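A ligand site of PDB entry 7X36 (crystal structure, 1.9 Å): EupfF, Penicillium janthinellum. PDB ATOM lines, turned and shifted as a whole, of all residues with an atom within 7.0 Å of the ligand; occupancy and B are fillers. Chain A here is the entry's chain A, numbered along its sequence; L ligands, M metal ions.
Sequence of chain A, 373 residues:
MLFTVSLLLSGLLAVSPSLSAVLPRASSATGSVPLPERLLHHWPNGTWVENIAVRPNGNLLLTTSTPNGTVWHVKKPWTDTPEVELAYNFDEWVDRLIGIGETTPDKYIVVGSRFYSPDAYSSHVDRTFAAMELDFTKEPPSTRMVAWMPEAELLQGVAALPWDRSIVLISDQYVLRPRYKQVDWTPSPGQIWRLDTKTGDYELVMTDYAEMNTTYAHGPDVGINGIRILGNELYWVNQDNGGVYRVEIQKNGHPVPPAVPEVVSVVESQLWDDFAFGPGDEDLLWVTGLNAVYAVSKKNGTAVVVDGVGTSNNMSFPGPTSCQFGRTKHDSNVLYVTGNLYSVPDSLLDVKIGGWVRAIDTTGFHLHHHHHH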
ATOM      1  N   TRP A  48      -2.655 -11.266 -30.161  1.00  0.00           N
ATOM      2  CA  TRP A  48      -1.351 -10.674 -30.452  1.00  0.00           C
ATOM      3  C   TRP A  48      -0.324 -11.798 -30.409  1.00  0.00           C
ATOM      4  O   TRP A  48      -0.016 -12.318 -29.337  1.00  0.00           O
ATOM      5  CB  TRP A  48      -1.082  -9.567 -29.419  1.00  0.00           C
ATOM      6  CG  TRP A  48       0.280  -8.946 -29.335  1.00  0.00           C
ATOM      7  CD1 TRP A  48       1.480  -9.459 -29.787  1.00  0.00           C
ATOM      8  CD2 TRP A  48       0.585  -7.673 -28.746  1.00  0.00           C
ATOM      9  NE1 TRP A  48       2.483  -8.593 -29.488  1.00  0.00           N
ATOM     10  CE2 TRP A  48       1.977  -7.492 -28.863  1.00  0.00           C
ATOM     11  CE3 TRP A  48      -0.183  -6.681 -28.127  1.00  0.00           C
ATOM     12  CZ2 TRP A  48       2.626  -6.332 -28.393  1.00  0.00           C
ATOM     13  CZ3 TRP A  48       0.461  -5.535 -27.649  1.00  0.00           C
ATOM     14  CH2 TRP A  48       1.861  -5.374 -27.787  1.00  0.00           C
ATOM     15  N   GLU A  50       3.371 -12.854 -30.592  1.00  0.00           N
ATOM     16  CA  GLU A  50       4.542 -12.054 -30.255  1.00  0.00           C
ATOM     17  C   GLU A  50       5.880 -12.706 -30.581  1.00  0.00           C
ATOM     18  O   GLU A  50       6.830 -11.999 -30.926  1.00  0.00           O
ATOM     19  CB  GLU A  50       4.494 -11.691 -28.769  1.00  0.00           C
ATOM     20  CG  GLU A  50       5.736 -11.027 -28.208  1.00  0.00           C
ATOM     21  CD  GLU A  50       6.129  -9.724 -28.889  1.00  0.00           C
ATOM     22  OE1 GLU A  50       7.257  -9.250 -28.627  1.00  0.00           O
ATOM     23  OE2 GLU A  50       5.333  -9.157 -29.679  1.00  0.00           O
ATOM     24  N   THR A  64       1.589 -15.834 -27.284  1.00  0.00           N
ATOM     25  CA  THR A  64       0.655 -14.725 -27.458  1.00  0.00           C
ATOM     26  C   THR A  64       0.720 -13.800 -26.250  1.00  0.00           C
ATOM     27  O   THR A  64       0.947 -14.239 -25.122  1.00  0.00           O
ATOM     28  CB  THR A  64      -0.796 -15.185 -27.628  1.00  0.00           C
ATOM     29  OG1 THR A  64      -1.273 -15.661 -26.363  1.00  0.00           O
ATOM     30  CG2 THR A  64      -0.902 -16.257 -28.711  1.00  0.00           C
ATOM     31  N   SER A  65       0.523 -12.513 -26.515  1.00  0.00           N
ATOM     32  CA  SER A  65       0.511 -11.502 -25.463  1.00  0.00           C
ATOM     33  C   SER A  65      -0.906 -11.174 -25.037  1.00  0.00           C
ATOM     34  O   SER A  65      -1.162 -10.946 -23.846  1.00  0.00           O
ATOM     35  CB  SER A  65       1.220 -10.235 -25.928  1.00  0.00           C
ATOM     36  OG  SER A  65       2.606 -10.478 -26.071  1.00  0.00           O
ATOM     37  N   THR A  66      -1.833 -11.131 -25.991  1.00  0.00           N
ATOM     38  CA  THR A  66      -3.244 -10.948 -25.719  1.00  0.00           C
ATOM     39  C   THR A  66      -4.017 -11.928 -26.579  1.00  0.00           C
ATOM     40  O   THR A  66      -3.505 -12.390 -27.610  1.00  0.00           O
ATOM     41  CB  THR A  66      -3.690  -9.494 -25.980  1.00  0.00           C
ATOM     42  OG1 THR A  66      -3.509  -9.176 -27.354  1.00  0.00           O
ATOM     43  CG2 THR A  66      -2.878  -8.506 -25.114  1.00  0.00           C
ATOM     44  N   ARG A  96       0.218 -12.008 -19.695  1.00  0.00           N
ATOM     45  CA  ARG A  96       0.787 -11.910 -21.046  1.00  0.00           C
ATOM     46  C   ARG A  96       2.063 -12.710 -21.125  1.00  0.00           C
ATOM     47  O   ARG A  96       2.787 -12.825 -20.128  1.00  0.00           O
ATOM     48  CB  ARG A  96       1.104 -10.468 -21.414  1.00  0.00           C
ATOM     49  CG  ARG A  96      -0.084  -9.486 -21.372  1.00  0.00           C
ATOM     50  CD  ARG A  96       0.144  -8.360 -22.355  1.00  0.00           C
ATOM     51  NE  ARG A  96      -0.942  -7.380 -22.387  1.00  0.00           N
ATOM     52  CZ  ARG A  96      -0.957  -6.324 -23.194  1.00  0.00           C
ATOM     53  NH1 ARG A  96       0.061  -6.127 -24.029  1.00  0.00           N
ATOM     54  NH2 ARG A  96      -1.971  -5.484 -23.177  1.00  0.00           N
ATOM     55  N   LEU A  97       2.364 -13.226 -22.334  1.00  0.00           N
ATOM     56  CA  LEU A  97       3.675 -13.788 -22.638  1.00  0.00           C
ATOM     57  C   LEU A  97       4.344 -12.941 -23.699  1.00  0.00           C
ATOM     58  O   LEU A  97       3.689 -12.331 -24.567  1.00  0.00           O
ATOM     59  CB  LEU A  97       3.634 -15.251 -23.147  1.00  0.00           C
ATOM     60  CG  LEU A  97       3.335 -16.358 -22.130  1.00  0.00           C
ATOM     61  CD1 LEU A  97       3.458 -17.713 -22.784  1.00  0.00           C
ATOM     62  CD2 LEU A  97       4.281 -16.228 -20.963  1.00  0.00           C
ATOM     63  N   ILE A  98       5.664 -12.901 -23.638  1.00  0.00           N
ATOM     64  CA  ILE A  98       6.365 -12.077 -24.612  1.00  0.00           C
ATOM     65  C   ILE A  98       7.288 -12.995 -25.423  1.00  0.00           C
ATOM     66  O   ILE A  98       6.820 -13.673 -26.349  1.00  0.00           O
ATOM     67  CB  ILE A  98       7.078 -10.898 -23.889  1.00  0.00           C
ATOM     68  CG1 ILE A  98       6.043 -10.226 -22.974  1.00  0.00           C
ATOM     69  CG2 ILE A  98       7.568  -9.855 -24.851  1.00  0.00           C
ATOM     70  CD1 ILE A  98       6.373  -8.764 -22.584  1.00  0.00           C
ATOM     71  N   GLY A  99       8.553 -13.106 -25.033  1.00  0.00           N
ATOM     72  CA  GLY A  99       9.493 -13.934 -25.764  1.00  0.00           C
ATOM     73  C   GLY A  99       9.483 -15.414 -25.364  1.00  0.00           C
ATOM     74  O   GLY A  99       8.906 -15.831 -24.364  1.00  0.00           O
ATOM     75  N   PHE A 115      -0.346  -7.340 -16.790  1.00  0.00           N
ATOM     76  CA  PHE A 115      -0.521  -6.093 -17.510  1.00  0.00           C
ATOM     77  C   PHE A 115      -1.792  -5.400 -17.041  1.00  0.00           C
ATOM     78  O   PHE A 115      -2.751  -6.059 -16.651  1.00  0.00           O
ATOM     79  CB  PHE A 115      -0.610  -6.327 -19.019  1.00  0.00           C
ATOM     80  CG  PHE A 115       0.719  -6.256 -19.733  1.00  0.00           C
ATOM     81  CD1 PHE A 115       1.708  -7.202 -19.484  1.00  0.00           C
ATOM     82  CD2 PHE A 115       0.966  -5.251 -20.657  1.00  0.00           C
ATOM     83  CE1 PHE A 115       2.926  -7.136 -20.171  1.00  0.00           C
ATOM     84  CE2 PHE A 115       2.190  -5.178 -21.364  1.00  0.00           C
ATOM     85  CZ  PHE A 115       3.173  -6.124 -21.107  1.00  0.00           C
ATOM     86  N   ALA A 120      -3.955  -2.846 -26.565  1.00  0.00           N
ATOM     87  CA  ALA A 120      -2.696  -2.891 -27.302  1.00  0.00           C
ATOM     88  C   ALA A 120      -1.667  -1.908 -26.775  1.00  0.00           C
ATOM     89  O   ALA A 120      -0.460  -2.122 -26.954  1.00  0.00           O
ATOM     90  CB  ALA A 120      -2.965  -2.643 -28.787  1.00  0.00           C
ATOM     91  N   SER A 122      -1.390  -0.940 -23.517  1.00  0.00           N
ATOM     92  CA  SER A 122      -1.275  -1.051 -22.068  1.00  0.00           C
ATOM     93  C   SER A 122       0.161  -1.297 -21.641  1.00  0.00           C
ATOM     94  O   SER A 122       0.898  -2.035 -22.296  1.00  0.00           O
ATOM     95  CB  SER A 122      -2.176  -2.177 -21.554  1.00  0.00           C
ATOM     96  OG  SER A 122      -1.914  -2.437 -20.176  1.00  0.00           O
ATOM     97  N   SER A 123       0.554  -0.690 -20.535  1.00  0.00           N
ATOM     98  CA  SER A 123       1.835  -1.002 -19.929  1.00  0.00           C
ATOM     99  C   SER A 123       1.743  -2.289 -19.140  1.00  0.00           C
ATOM    100  O   SER A 123       0.638  -2.788 -18.854  1.00  0.00           O
ATOM    101  CB  SER A 123       2.287   0.128 -19.018  1.00  0.00           C
ATOM    102  OG  SER A 123       2.297   1.353 -19.721  1.00  0.00           O
ATOM    103  N   HIS A 124       2.900  -2.800 -18.739  1.00  0.00           N
ATOM    104  CA  HIS A 124       2.941  -3.915 -17.801  1.00  0.00           C
ATOM    105  C   HIS A 124       2.682  -3.395 -16.382  1.00  0.00           C
ATOM    106  O   HIS A 124       2.634  -2.192 -16.133  1.00  0.00           O
ATOM    107  CB  HIS A 124       4.297  -4.586 -17.849  1.00  0.00           C
ATOM    108  CG  HIS A 124       5.426  -3.651 -17.588  1.00  0.00           C
ATOM    109  ND1 HIS A 124       5.736  -2.596 -18.422  1.00  0.00           N
ATOM    110  CD2 HIS A 124       6.347  -3.610 -16.584  1.00  0.00           C
ATOM    111  CE1 HIS A 124       6.785  -1.945 -17.947  1.00  0.00           C
ATOM    112  NE2 HIS A 124       7.188  -2.555 -16.844  1.00  0.00           N
ATOM    113  N   LEU A 154      11.044  -5.004 -18.158  1.00  0.00           N
ATOM    114  CA  LEU A 154      10.144  -5.762 -19.043  1.00  0.00           C
ATOM    115  C   LEU A 154      10.954  -6.806 -19.809  1.00  0.00           C
ATOM    116  O   LEU A 154      11.771  -6.454 -20.678  1.00  0.00           O
ATOM    117  CB  LEU A 154       9.381  -4.822 -19.978  1.00  0.00           C
ATOM    118  CG  LEU A 154       8.568  -5.487 -21.094  1.00  0.00           C
ATOM    119  CD1 LEU A 154       7.175  -4.877 -21.216  1.00  0.00           C
ATOM    120  CD2 LEU A 154       9.342  -5.445 -22.442  1.00  0.00           C
ATOM    121  N   LEU A 155      10.749  -8.073 -19.498  1.00  0.00           N
ATOM    122  CA  LEU A 155      11.481  -9.122 -20.186  1.00  0.00           C
ATOM    123  C   LEU A 155      10.935  -9.304 -21.590  1.00  0.00           C
ATOM    124  O   LEU A 155       9.715  -9.358 -21.814  1.00  0.00           O
ATOM    125  CB  LEU A 155      11.409 -10.435 -19.421  1.00  0.00           C
ATOM    126  CG  LEU A 155      11.918 -10.383 -17.988  1.00  0.00           C
ATOM    127  CD1 LEU A 155      11.725 -11.762 -17.333  1.00  0.00           C
ATOM    128  CD2 LEU A 155      13.381  -9.933 -17.974  1.00  0.00           C
ATOM    129  N   GLN A 156      11.848  -9.420 -22.560  1.00  0.00           N
ATOM    130  CA  GLN A 156      11.501  -9.332 -23.962  1.00  0.00           C
ATOM    131  C   GLN A 156      11.931 -10.574 -24.740  1.00  0.00           C
ATOM    132  O   GLN A 156      11.101 -11.434 -25.031  1.00  0.00           O
ATOM    133  CB  GLN A 156      12.123  -8.073 -24.557  1.00  0.00           C
ATOM    134  CG  GLN A 156      11.909  -7.894 -26.042  1.00  0.00           C
ATOM    135  CD  GLN A 156      10.472  -7.579 -26.378  1.00  0.00           C
ATOM    136  OE1 GLN A 156       9.768  -8.414 -26.925  1.00  0.00           O
ATOM    137  NE2 GLN A 156      10.033  -6.370 -26.050  1.00  0.00           N
ATOM    138  N   GLN A 173      13.713  -4.035 -21.600  1.00  0.00           N
ATOM    139  CA  GLN A 173      13.577  -2.580 -21.672  1.00  0.00           C
ATOM    140  C   GLN A 173      12.136  -2.217 -21.945  1.00  0.00           C
ATOM    141  O   GLN A 173      11.519  -2.787 -22.842  1.00  0.00           O
ATOM    142  CB  GLN A 173      14.482  -1.972 -22.764  1.00  0.00           C
ATOM    143  CG  GLN A 173      14.664  -0.440 -22.624  1.00  0.00           C
ATOM    144  CD  GLN A 173      13.420   0.343 -23.002  1.00  0.00           C
ATOM    145  OE1 GLN A 173      12.699  -0.032 -23.932  1.00  0.00           O
ATOM    146  NE2 GLN A 173      13.130   1.414 -22.251  1.00  0.00           N
ATOM    147  N   TYR A 174      11.588  -1.285 -21.134  1.00  0.00           N
ATOM    148  CA  TYR A 174      10.395  -0.515 -21.461  1.00  0.00           C
ATOM    149  C   TYR A 174      10.253   0.641 -20.464  1.00  0.00           C
ATOM    150  O   TYR A 174      11.259   1.019 -19.833  1.00  0.00           O
ATOM    151  CB  TYR A 174       9.150  -1.416 -21.481  1.00  0.00           C
ATOM    152  CG  TYR A 174       7.966  -0.787 -22.175  1.00  0.00           C
ATOM    153  CD1 TYR A 174       8.108  -0.085 -23.359  1.00  0.00           C
ATOM    154  CD2 TYR A 174       6.700  -0.839 -21.588  1.00  0.00           C
ATOM    155  CE1 TYR A 174       7.019   0.518 -23.967  1.00  0.00           C
ATOM    156  CE2 TYR A 174       5.618  -0.257 -22.192  1.00  0.00           C
ATOM    157  CZ  TYR A 174       5.771   0.424 -23.356  1.00  0.00           C
ATOM    158  OH  TYR A 174       4.652   1.010 -23.925  1.00  0.00           O
ATOM    159  N   ASP A 221       7.874   2.999 -27.763  1.00  0.00           N
ATOM    160  CA  ASP A 221       8.467   1.765 -28.276  1.00  0.00           C
ATOM    161  C   ASP A 221       9.435   1.240 -27.225  1.00  0.00           C
ATOM    162  O   ASP A 221       9.432   1.712 -26.079  1.00  0.00           O
ATOM    163  CB  ASP A 221       9.159   2.002 -29.639  1.00  0.00           C
ATOM    164  CG  ASP A 221      10.365   2.922 -29.535  1.00  0.00           C
ATOM    165  OD1 ASP A 221      10.669   3.413 -28.428  1.00  0.00           O
ATOM    166  OD2 ASP A 221      11.043   3.167 -30.580  1.00  0.00           O
ATOM    167  N   VAL A 222      10.255   0.274 -27.613  1.00  0.00           N
ATOM    168  CA  VAL A 222      11.341  -0.221 -26.773  1.00  0.00           C
ATOM    169  C   VAL A 222      12.669   0.132 -27.424  1.00  0.00           C
ATOM    170  O   VAL A 222      12.724   0.498 -28.591  1.00  0.00           O
ATOM    171  CB  VAL A 222      11.264  -1.736 -26.528  1.00  0.00           C
ATOM    172  CG1 VAL A 222       9.973  -2.092 -25.671  1.00  0.00           C
ATOM    173  CG2 VAL A 222      11.338  -2.520 -27.863  1.00  0.00           C
ATOM    174  N   ASN A 225      15.235  -5.035 -28.315  1.00  0.00           N
ATOM    175  CA  ASN A 225      14.076  -5.909 -28.481  1.00  0.00           C
ATOM    176  C   ASN A 225      14.594  -7.354 -28.569  1.00  0.00           C
ATOM    177  O   ASN A 225      15.102  -7.880 -27.570  1.00  0.00           O
ATOM    178  CB  ASN A 225      13.250  -5.447 -29.691  1.00  0.00           C
ATOM    179  CG  ASN A 225      11.769  -5.865 -29.603  1.00  0.00           C
ATOM    180  OD1 ASN A 225      11.478  -6.919 -29.083  1.00  0.00           O
ATOM    181  ND2 ASN A 225      10.866  -5.044 -30.134  1.00  0.00           N
ATOM    182  N   GLN A 239      14.858  -1.309 -31.545  1.00  0.00           N
ATOM    183  CA  GLN A 239      13.628  -0.880 -32.197  1.00  0.00           C
ATOM    184  C   GLN A 239      13.601   0.631 -32.421  1.00  0.00           C
ATOM    185  O   GLN A 239      12.869   1.104 -33.292  1.00  0.00           O
ATOM    186  CB  GLN A 239      12.397  -1.290 -31.346  1.00  0.00           C
ATOM    187  CG  GLN A 239      11.025  -0.945 -31.985  1.00  0.00           C
ATOM    188  CD  GLN A 239       9.853  -1.638 -31.331  1.00  0.00           C
ATOM    189  OE1 GLN A 239       9.463  -1.294 -30.211  1.00  0.00           O
ATOM    190  NE2 GLN A 239       9.259  -2.608 -32.039  1.00  0.00           N
ATOM    191  N   ASP A 273      12.052  -5.773 -34.514  1.00  0.00           N
ATOM    192  CA  ASP A 273      11.448  -6.526 -33.412  1.00  0.00           C
ATOM    193  C   ASP A 273      12.259  -7.784 -33.075  1.00  0.00           C
ATOM    194  O   ASP A 273      12.920  -7.796 -32.034  1.00  0.00           O
ATOM    195  CB  ASP A 273       9.986  -6.814 -33.734  1.00  0.00           C
ATOM    196  CG  ASP A 273       9.165  -7.032 -32.494  1.00  0.00           C
ATOM    197  OD1 ASP A 273       9.769  -7.484 -31.506  1.00  0.00           O
ATOM    198  OD2 ASP A 273       7.942  -6.773 -32.503  1.00  0.00           O
ATOM    199  N   ASN A 340       1.190  -9.436 -35.447  1.00  0.00           N
ATOM    200  CA  ASN A 340       0.138  -9.162 -34.475  1.00  0.00           C
ATOM    201  C   ASN A 340      -0.929  -8.180 -34.936  1.00  0.00           C
ATOM    202  O   ASN A 340      -1.846  -7.904 -34.151  1.00  0.00           O
ATOM    203  CB  ASN A 340       0.734  -8.666 -33.144  1.00  0.00           C
ATOM    204  CG  ASN A 340       1.414  -7.315 -33.260  1.00  0.00           C
ATOM    205  OD1 ASN A 340       1.639  -6.795 -34.363  1.00  0.00           O
ATOM    206  ND2 ASN A 340       1.754  -6.739 -32.109  1.00  0.00           N
HETATM  207  C1  LIG L   1       3.861  -7.352 -25.454  1.00  0.00           C
HETATM  208  O1  LIG L   1       4.176  -8.295 -26.218  1.00  0.00           O
HETATM  209  O2  LIG L   1       2.785  -7.462 -24.823  1.00  0.00           O
HETATM  210  C2  LIG L   1       4.742  -6.119 -25.332  1.00  0.00           C
HETATM  211  C3  LIG L   1       4.270  -4.939 -24.741  1.00  0.00           C
HETATM  212  C4  LIG L   1       5.087  -3.807 -24.648  1.00  0.00           C
HETATM  213  C5  LIG L   1       6.394  -3.847 -25.158  1.00  0.00           C
HETATM  214  C6  LIG L   1       6.861  -5.014 -25.765  1.00  0.00           C
HETATM  215  C7  LIG L   1       6.038  -6.146 -25.850  1.00  0.00           C
HETATM  216 CA    CA M   1       9.472  -8.540 -29.233  1.00  0.00          CA
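OG of Ser 65 lies within hydrogen-bond range of O1 of the ligand.
The guanidinium group (NH1) of Arg 96 is in salt-bridge range of an oxygen (O2) of the ligand, 3.1 Å away.
The indole nitrogen (NE1) of Trp 48 lies within hydrogen-bond range of the side-chain carboxylate (OE2) of Glu 50 (2.9 Å).
The backbone NH (N) of Trp 48 sits at hydrogen-bond distance from the backbone carbonyl oxygen (O) of Thr 66.
O of Trp 48 lies within hydrogen-bond range of N of Ser 65, at 2.9 Å.
The indole nitrogen (NE1) of Trp 48 lies close to the side-chain amide nitrogen (ND2) of Asn 340, at 3.3 Å.
N of Gly 99 is in hydrogen-bond range of O of Gln 156, 3.0 Å away.
The backbone carbonyl oxygen (O) of Leu 97 sits at hydrogen-bond distance from the side-chain hydroxyl (OG) of Ser 65 (2.6 Å).
CZ2 of Trp 48 touches O1 of the ligand, 3.3 Å away.
Glu 50 touches the ligand (CD to O1, 3.6 Å).
Ile 98 touches the ligand (CG2 to O1, 3.98 Å).
CZ of Phe 115 touches O2 of the ligand, at 3.97 Å.
NE2 of Gln 156 touches C6 of the ligand, 3.5 Å away.
The nearest printed residue that does not touch the ligand is Val 222 (4.02 Å).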
